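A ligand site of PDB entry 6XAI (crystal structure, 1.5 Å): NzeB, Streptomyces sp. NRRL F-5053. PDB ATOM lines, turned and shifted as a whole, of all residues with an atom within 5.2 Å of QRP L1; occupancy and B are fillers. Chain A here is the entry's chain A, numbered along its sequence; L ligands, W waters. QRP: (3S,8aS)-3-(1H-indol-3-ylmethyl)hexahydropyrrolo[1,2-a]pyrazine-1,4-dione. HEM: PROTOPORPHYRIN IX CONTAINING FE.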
ATOM      1  N   GLN A  75     -21.590   9.626 -21.252  1.00  0.00           N
ATOM      2  CA  GLN A  75     -21.808  10.864 -20.515  1.00  0.00           C
ATOM      3  C   GLN A  75     -21.015  12.028 -21.086  1.00  0.00           C
ATOM      4  O   GLN A  75     -21.421  13.193 -20.947  1.00  0.00           O
ATOM      5  CB  GLN A  75     -21.437  10.656 -19.043  1.00  0.00           C
ATOM      6  CG  GLN A  75     -19.958  10.396 -18.814  1.00  0.00           C
ATOM      7  CD  GLN A  75     -19.657   9.702 -17.494  1.00  0.00           C
ATOM      8  OE1 GLN A  75     -19.664  10.343 -16.432  1.00  0.00           O
ATOM      9  NE2 GLN A  75     -19.331   8.396 -17.545  1.00  0.00           N
ATOM     10  N   GLU A  76     -19.862  11.746 -21.746  1.00  0.00           N
ATOM     11  CA  GLU A  76     -18.975  12.808 -22.215  1.00  0.00           C
ATOM     12  C   GLU A  76     -19.481  13.380 -23.548  1.00  0.00           C
ATOM     13  O   GLU A  76     -19.981  12.647 -24.407  1.00  0.00           O
ATOM     14  CB  GLU A  76     -17.530  12.275 -22.368  1.00  0.00           C
ATOM     15  CG  GLU A  76     -17.330  11.153 -23.386  1.00  0.00           C
ATOM     16  CD  GLU A  76     -17.471   9.739 -22.800  1.00  0.00           C
ATOM     17  OE1 GLU A  76     -18.137   9.570 -21.761  1.00  0.00           O
ATOM     18  OE2 GLU A  76     -16.946   8.774 -23.398  1.00  0.00           O
ATOM     19  N   LEU A  80     -13.375  10.569 -26.272  1.00  0.00           N
ATOM     20  CA  LEU A  80     -12.082  10.804 -25.639  1.00  0.00           C
ATOM     21  C   LEU A  80     -10.963  10.185 -26.478  1.00  0.00           C
ATOM     22  O   LEU A  80     -10.202   9.327 -26.040  1.00  0.00           O
ATOM     23  CB  LEU A  80     -12.074  10.268 -24.212  1.00  0.00           C
ATOM     24  CG  LEU A  80     -13.247  10.740 -23.333  1.00  0.00           C
ATOM     25  CD1 LEU A  80     -13.158  10.166 -21.902  1.00  0.00           C
ATOM     26  CD2 LEU A  80     -13.354  12.272 -23.342  1.00  0.00           C
ATOM     27  N   PHE A 177     -17.207  18.505 -19.292  1.00  0.00           N
ATOM     28  CA  PHE A 177     -18.600  18.338 -19.674  1.00  0.00           C
ATOM     29  C   PHE A 177     -19.189  19.583 -20.332  1.00  0.00           C
ATOM     30  O   PHE A 177     -20.194  19.482 -21.039  1.00  0.00           O
ATOM     31  CB  PHE A 177     -19.441  18.024 -18.448  1.00  0.00           C
ATOM     32  CG  PHE A 177     -19.284  16.612 -17.940  1.00  0.00           C
ATOM     33  CD1 PHE A 177     -19.815  15.545 -18.660  1.00  0.00           C
ATOM     34  CD2 PHE A 177     -18.626  16.367 -16.747  1.00  0.00           C
ATOM     35  CE1 PHE A 177     -19.719  14.251 -18.194  1.00  0.00           C
ATOM     36  CE2 PHE A 177     -18.503  15.071 -16.259  1.00  0.00           C
ATOM     37  CZ  PHE A 177     -19.050  14.007 -16.979  1.00  0.00           C
ATOM     38  N   THR A 244      -6.179  14.012 -12.789  1.00  0.00           N
ATOM     39  CA  THR A 244      -6.530  13.247 -11.603  1.00  0.00           C
ATOM     40  C   THR A 244      -5.636  13.625 -10.432  1.00  0.00           C
ATOM     41  O   THR A 244      -6.117  13.968  -9.338  1.00  0.00           O
ATOM     42  CB  THR A 244      -6.380  11.748 -11.901  1.00  0.00           C
ATOM     43  OG1 THR A 244      -5.075  11.517 -12.456  1.00  0.00           O
ATOM     44  CG2 THR A 244      -7.444  11.291 -12.896  1.00  0.00           C
ATOM     45  N   LEU A 286     -13.669  13.696  -6.380  1.00  0.00           N
ATOM     46  CA  LEU A 286     -12.778  13.964  -7.505  1.00  0.00           C
ATOM     47  C   LEU A 286     -13.558  14.088  -8.804  1.00  0.00           C
ATOM     48  O   LEU A 286     -13.839  15.211  -9.261  1.00  0.00           O
ATOM     49  CB  LEU A 286     -11.672  12.917  -7.603  1.00  0.00           C
ATOM     50  CG  LEU A 286     -10.654  13.174  -8.720  1.00  0.00           C
ATOM     51  CD1 LEU A 286     -10.031  14.589  -8.697  1.00  0.00           C
ATOM     52  CD2 LEU A 286      -9.566  12.091  -8.708  1.00  0.00           C
ATOM     53  N   SER A 287     -13.984  12.962  -9.383  1.00  0.00           N
ATOM     54  CA  SER A 287     -14.722  13.039 -10.631  1.00  0.00           C
ATOM     55  C   SER A 287     -16.114  13.640 -10.422  1.00  0.00           C
ATOM     56  O   SER A 287     -16.787  13.370  -9.423  1.00  0.00           O
ATOM     57  CB  SER A 287     -14.862  11.658 -11.257  1.00  0.00           C
ATOM     58  OG  SER A 287     -15.542  11.735 -12.501  1.00  0.00           O
ATOM     59  N   THR A 288     -16.537  14.454 -11.384  1.00  0.00           N
ATOM     60  CA  THR A 288     -17.919  14.941 -11.483  1.00  0.00           C
ATOM     61  C   THR A 288     -18.781  14.025 -12.341  1.00  0.00           C
ATOM     62  O   THR A 288     -19.979  14.273 -12.508  1.00  0.00           O
ATOM     63  CB  THR A 288     -17.936  16.365 -12.058  1.00  0.00           C
ATOM     64  OG1 THR A 288     -17.361  16.347 -13.381  1.00  0.00           O
ATOM     65  CG2 THR A 288     -17.124  17.322 -11.154  1.00  0.00           C
ATOM     66  N   GLY A 289     -18.193  12.984 -12.923  1.00  0.00           N
ATOM     67  CA  GLY A 289     -18.953  11.984 -13.641  1.00  0.00           C
ATOM     68  C   GLY A 289     -18.861  10.653 -12.922  1.00  0.00           C
ATOM     69  O   GLY A 289     -18.691  10.607 -11.692  1.00  0.00           O
ATOM     70  N   SER A 290     -18.949   9.556 -13.682  1.00  0.00           N
ATOM     71  CA  SER A 290     -19.046   8.228 -13.118  1.00  0.00           C
ATOM     72  C   SER A 290     -18.173   7.253 -13.890  1.00  0.00           C
ATOM     73  O   SER A 290     -17.954   7.410 -15.096  1.00  0.00           O
ATOM     74  CB  SER A 290     -20.496   7.725 -13.234  1.00  0.00           C
ATOM     75  OG  SER A 290     -21.357   8.410 -12.331  1.00  0.00           O
ATOM     76  N   VAL A 291     -17.670   6.238 -13.179  1.00  0.00           N
ATOM     77  CA  VAL A 291     -17.146   5.076 -13.877  1.00  0.00           C
ATOM     78  C   VAL A 291     -18.309   4.421 -14.603  1.00  0.00           C
ATOM     79  O   VAL A 291     -19.466   4.538 -14.184  1.00  0.00           O
ATOM     80  CB  VAL A 291     -16.462   4.083 -12.932  1.00  0.00           C
ATOM     81  CG1 VAL A 291     -15.307   4.729 -12.179  1.00  0.00           C
ATOM     82  CG2 VAL A 291     -17.463   3.481 -11.977  1.00  0.00           C
ATOM     83  N   LYS A 292     -18.022   3.694 -15.683  1.00  0.00           N
ATOM     84  CA  LYS A 292     -19.127   3.140 -16.444  1.00  0.00           C
ATOM     85  C   LYS A 292     -18.730   1.836 -17.135  1.00  0.00           C
ATOM     86  O   LYS A 292     -17.550   1.584 -17.417  1.00  0.00           O
ATOM     87  CB  LYS A 292     -19.746   4.169 -17.404  1.00  0.00           C
ATOM     88  CG  LYS A 292     -19.004   4.367 -18.734  1.00  0.00           C
ATOM     89  CD  LYS A 292     -17.603   4.893 -18.528  1.00  0.00           C
ATOM     90  CE  LYS A 292     -16.993   5.311 -19.837  1.00  0.00           C
ATOM     91  NZ  LYS A 292     -15.546   5.577 -19.696  1.00  0.00           N
ATOM     92  N   LEU A 316     -18.562   7.291  -7.971  1.00  0.00           N
ATOM     93  CA  LEU A 316     -17.716   6.902  -6.849  1.00  0.00           C
ATOM     94  C   LEU A 316     -17.987   7.794  -5.647  1.00  0.00           C
ATOM     95  O   LEU A 316     -17.931   7.339  -4.498  1.00  0.00           O
ATOM     96  CB  LEU A 316     -16.252   6.974  -7.246  1.00  0.00           C
ATOM     97  CG  LEU A 316     -15.897   6.128  -8.468  1.00  0.00           C
ATOM     98  CD1 LEU A 316     -14.400   6.208  -8.713  1.00  0.00           C
ATOM     99  CD2 LEU A 316     -16.327   4.686  -8.273  1.00  0.00           C
ATOM    100  N   GLY A 343     -12.497   5.216  -3.929  1.00  0.00           N
ATOM    101  CA  GLY A 343     -11.751   6.319  -4.555  1.00  0.00           C
ATOM    102  C   GLY A 343     -10.890   5.900  -5.724  1.00  0.00           C
ATOM    103  O   GLY A 343     -10.596   6.728  -6.606  1.00  0.00           O
ATOM    104  N   PHE A 390     -14.116  17.083 -15.781  1.00  0.00           N
ATOM    105  CA  PHE A 390     -14.342  15.731 -15.263  1.00  0.00           C
ATOM    106  C   PHE A 390     -13.748  15.580 -13.865  1.00  0.00           C
ATOM    107  O   PHE A 390     -14.312  14.888 -13.003  1.00  0.00           O
ATOM    108  CB  PHE A 390     -13.666  14.680 -16.144  1.00  0.00           C
ATOM    109  CG  PHE A 390     -14.237  14.529 -17.539  1.00  0.00           C
ATOM    110  CD1 PHE A 390     -15.378  15.206 -17.933  1.00  0.00           C
ATOM    111  CD2 PHE A 390     -13.617  13.674 -18.438  1.00  0.00           C
ATOM    112  CE1 PHE A 390     -15.891  15.047 -19.246  1.00  0.00           C
ATOM    113  CE2 PHE A 390     -14.119  13.516 -19.728  1.00  0.00           C
ATOM    114  CZ  PHE A 390     -15.246  14.208 -20.135  1.00  0.00           C
ATOM    115  N   PHE A 391     -12.573  16.168 -13.652  1.00  0.00           N
ATOM    116  CA  PHE A 391     -11.836  16.007 -12.393  1.00  0.00           C
ATOM    117  C   PHE A 391     -11.727  17.369 -11.706  1.00  0.00           C
ATOM    118  O   PHE A 391     -11.000  18.253 -12.186  1.00  0.00           O
ATOM    119  CB  PHE A 391     -10.485  15.342 -12.664  1.00  0.00           C
ATOM    120  CG  PHE A 391     -10.621  14.052 -13.407  1.00  0.00           C
ATOM    121  CD1 PHE A 391     -11.229  12.959 -12.806  1.00  0.00           C
ATOM    122  CD2 PHE A 391     -10.211  13.955 -14.723  1.00  0.00           C
ATOM    123  CE1 PHE A 391     -11.395  11.773 -13.469  1.00  0.00           C
ATOM    124  CE2 PHE A 391     -10.366  12.749 -15.421  1.00  0.00           C
ATOM    125  CZ  PHE A 391     -10.964  11.657 -14.798  1.00  0.00           C
HETATM  126  C   QRP L   1     -14.802   8.204 -16.813  1.00  0.00           C
HETATM  127  N   QRP L   1     -14.733   9.769 -14.957  1.00  0.00           N
HETATM  128  O   QRP L   1     -14.909   7.040 -17.165  1.00  0.00           O
HETATM  129  CA  QRP L   1     -14.153   8.537 -15.490  1.00  0.00           C
HETATM  130  CB  QRP L   1     -14.261   7.429 -14.429  1.00  0.00           C
HETATM  131  CG  QRP L   1     -13.697   7.957 -13.133  1.00  0.00           C
HETATM  132  OAA QRP L   1     -15.364  11.930 -15.234  1.00  0.00           O
HETATM  133  CAH QRP L   1     -16.364  10.511 -19.193  1.00  0.00           C
HETATM  134  CAI QRP L   1     -16.303  11.283 -17.887  1.00  0.00           C
HETATM  135  CAJ QRP L   1     -15.930   9.086 -18.844  1.00  0.00           C
HETATM  136  CAN QRP L   1     -15.099  10.823 -15.685  1.00  0.00           C
HETATM  137  CAT QRP L   1     -15.115  10.625 -17.177  1.00  0.00           C
HETATM  138  NAU QRP L   1     -15.244   9.221 -17.562  1.00  0.00           N
HETATM  139  CD1 QRP L   1     -14.459   8.273 -12.018  1.00  0.00           C
HETATM  140  CD2 QRP L   1     -12.379   8.269 -12.793  1.00  0.00           C
HETATM  141  NE1 QRP L   1     -13.640   8.730 -11.033  1.00  0.00           N
HETATM  142  CE2 QRP L   1     -12.378   8.752 -11.489  1.00  0.00           C
HETATM  143  CE3 QRP L   1     -11.209   8.157 -13.509  1.00  0.00           C
HETATM  144  CH2 QRP L   1      -9.993   9.026 -11.636  1.00  0.00           C
HETATM  145  CZ2 QRP L   1     -11.167   9.125 -10.899  1.00  0.00           C
HETATM  146  CZ3 QRP L   1     -10.010   8.546 -12.940  1.00  0.00           C
HETATM  147  CHA HEM L   2      -8.077   4.069 -13.424  1.00  0.00           C
HETATM  148  CHB HEM L   2      -8.557   7.046  -9.620  1.00  0.00           C
HETATM  149  CHC HEM L   2      -4.031   8.599 -10.365  1.00  0.00           C
HETATM  150  CHD HEM L   2      -3.533   5.602 -14.140  1.00  0.00           C
HETATM  151  C1A HEM L   2      -8.613   4.700 -12.337  1.00  0.00           C
HETATM  152  C2A HEM L   2      -9.920   4.472 -11.750  1.00  0.00           C
HETATM  153  C3A HEM L   2     -10.025   5.306 -10.710  1.00  0.00           C
HETATM  154  C4A HEM L   2      -8.810   6.086 -10.578  1.00  0.00           C
HETATM  155  CMA HEM L   2     -11.251   5.479  -9.804  1.00  0.00           C
HETATM  156  CAA HEM L   2     -10.981   3.454 -12.207  1.00  0.00           C
HETATM  157  CBA HEM L   2     -11.773   3.833 -13.454  1.00  0.00           C
HETATM  158  CGA HEM L   2     -12.802   2.789 -13.825  1.00  0.00           C
HETATM  159  O1A HEM L   2     -13.121   1.945 -12.952  1.00  0.00           O
HETATM  160  O2A HEM L   2     -13.303   2.811 -14.987  1.00  0.00           O
HETATM  161  C1B HEM L   2      -7.382   7.753  -9.487  1.00  0.00           C
HETATM  162  C2B HEM L   2      -7.090   8.784  -8.503  1.00  0.00           C
HETATM  163  C3B HEM L   2      -5.832   9.229  -8.736  1.00  0.00           C
HETATM  164  C4B HEM L   2      -5.308   8.461  -9.858  1.00  0.00           C
HETATM  165  CMB HEM L   2      -8.091   9.249  -7.420  1.00  0.00           C
HETATM  166  CAB HEM L   2      -5.015  10.310  -7.982  1.00  0.00           C
HETATM  167  CBB HEM L   2      -5.230  10.598  -6.694  1.00  0.00           C
HETATM  168  C1C HEM L   2      -3.494   7.908 -11.426  1.00  0.00           C
HETATM  169  C2C HEM L   2      -2.138   8.068 -11.926  1.00  0.00           C
HETATM  170  C3C HEM L   2      -2.000   7.257 -12.971  1.00  0.00           C
HETATM  171  C4C HEM L   2      -3.258   6.553 -13.174  1.00  0.00           C
HETATM  172  CMC HEM L   2      -1.089   9.027 -11.338  1.00  0.00           C
HETATM  173  CAC HEM L   2      -0.684   7.141 -13.783  1.00  0.00           C
HETATM  174  CBC HEM L   2      -0.629   6.566 -14.980  1.00  0.00           C
HETATM  175  C1D HEM L   2      -4.751   4.999 -14.350  1.00  0.00           C
HETATM  176  C2D HEM L   2      -5.151   4.228 -15.495  1.00  0.00           C
HETATM  177  C3D HEM L   2      -6.417   3.794 -15.290  1.00  0.00           C
HETATM  178  C4D HEM L   2      -6.845   4.301 -14.015  1.00  0.00           C
HETATM  179  CMD HEM L   2      -4.228   3.964 -16.717  1.00  0.00           C
HETATM  180  CAD HEM L   2      -7.315   2.950 -16.239  1.00  0.00           C
HETATM  181  CBD HEM L   2      -7.400   1.509 -15.764  1.00  0.00           C
HETATM  182  CGD HEM L   2      -8.380   0.735 -16.624  1.00  0.00           C
HETATM  183  O1D HEM L   2      -9.283   1.336 -17.266  1.00  0.00           O
HETATM  184  O2D HEM L   2      -8.280  -0.510 -16.652  1.00  0.00           O
HETATM  185  NA  HEM L   2      -7.960   5.661 -11.592  1.00  0.00           N
HETATM  186  NB  HEM L   2      -6.277   7.590 -10.295  1.00  0.00           N
HETATM  187  NC  HEM L   2      -4.143   6.961 -12.191  1.00  0.00           N
HETATM  188  ND  HEM L   2      -5.826   5.043 -13.466  1.00  0.00           N
HETATM  189 FE   HEM L   2      -5.943   6.103 -11.701  1.00  0.00          FE
HETATM  190  C   QRP L   3     -11.727   5.181 -19.782  1.00  0.00           C
HETATM  191  N   QRP L   3      -9.935   3.773 -18.761  1.00  0.00           N
HETATM  192  O   QRP L   3     -12.878   5.582 -19.854  1.00  0.00           O
HETATM  193  CA  QRP L   3     -11.304   4.280 -18.660  1.00  0.00           C
HETATM  194  CB  QRP L   3     -11.569   5.059 -17.349  1.00  0.00           C
HETATM  195  CG  QRP L   3     -10.624   6.225 -17.114  1.00  0.00           C
HETATM  196  OAA QRP L   3      -7.866   3.763 -19.643  1.00  0.00           O
HETATM  197  CAH QRP L   3      -9.645   7.318 -21.627  1.00  0.00           C
HETATM  198  CAI QRP L   3      -8.728   6.369 -20.841  1.00  0.00           C
HETATM  199  CAJ QRP L   3     -11.030   6.683 -21.615  1.00  0.00           C
HETATM  200  CAN QRP L   3      -9.035   4.149 -19.675  1.00  0.00           C
HETATM  201  CAT QRP L   3      -9.483   5.044 -20.784  1.00  0.00           C
HETATM  202  NAU QRP L   3     -10.831   5.573 -20.681  1.00  0.00           N
HETATM  203  CD1 QRP L   3      -9.471   6.164 -16.354  1.00  0.00           C
HETATM  204  CD2 QRP L   3     -10.725   7.535 -17.551  1.00  0.00           C
HETATM  205  NE1 QRP L   3      -8.890   7.383 -16.335  1.00  0.00           N
HETATM  206  CE2 QRP L   3      -9.636   8.246 -17.069  1.00  0.00           C
HETATM  207  CE3 QRP L   3     -11.697   8.161 -18.340  1.00  0.00           C
HETATM  208  CH2 QRP L   3     -10.441  10.231 -18.167  1.00  0.00           C
HETATM  209  CZ2 QRP L   3      -9.487   9.595 -17.387  1.00  0.00           C
HETATM  210  CZ3 QRP L   3     -11.542   9.517 -18.643  1.00  0.00           C
HETATM  211  O   HOH W   1      -6.948   7.956 -14.166  1.00  0.00           O
HETATM  212  O   HOH W   2     -17.222   9.006 -10.006  1.00  0.00           O
HETATM  213  O   HOH W   3     -13.755  10.083  -8.532  1.00  0.00           O
HETATM  214  O   HOH W   4     -15.059   4.265 -16.373  1.00  0.00           O
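The side-chain hydroxyl (OG) of Ser 287 sits at hydrogen-bond distance from an oxygen (OAA) of QRP L1, at 2.7 Å. NZ of Lys 292 is in hydrogen-bond range of O of QRP L1, at 3.0 Å. O of QRP L3 sits at hydrogen-bond distance from NZ of Lys 292 (2.7 Å).
An oxygen (O1D) of HEM L2 is in hydrogen-bond range of a nitrogen (N) of QRP L3 (2.9 Å).
OG of Ser 287 lies close to O of Phe 390 (3.4 Å). The side-chain hydroxyl (OG) of Ser 287 sits at hydrogen-bond distance from the backbone NH (N) of Gly 289, 3.0 Å away. The backbone carbonyl oxygen (O) of Phe 390 lies within hydrogen-bond range of the backbone NH (N) of Thr 288, 2.8 Å away. OE1 of Gln 75 lies within hydrogen-bond range of N of Ser 290 (2.9 Å).
Residues that only touch QRP L1: Glu 76 (3.3 Å), Phe 390 (3.4 Å), Leu 316 (3.5 Å), Phe 391 (3.6 Å), Gln 75 (3.6 Å), Thr 244 (3.6 Å), Val 291 (3.6 Å), Ser 290 (3.7 Å), Gly 289 (3.8 Å) and Phe 177 (3.97 Å). Hydrophobic or aromatic side chains within 4 Å of QRP L1: Phe 177, Val 291, Leu 316, Phe 390 and Phe 391. Within 4 Å of QRP L1: Gln 75, Glu 76, Phe 177, Thr 244, Ser 287, Gly 289, Ser 290, Val 291, Lys 292, Leu 316, Phe 390 and Phe 391.
Water W3 lies within hydrogen-bond range of a nitrogen (NE1) of QRP L1 and the backbone NH of Ser 287. Water W4 lies within hydrogen-bond range of O2A of HEM L2 (2.7 Å), O of QRP L1 (2.9 Å) and N of Lys 292 (3.1 Å). Water W2 lies within hydrogen-bond range of the backbone carbonyl oxygen of Gly 289 (2.8 Å) and the backbone NH of Leu 316 (3.0 Å).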
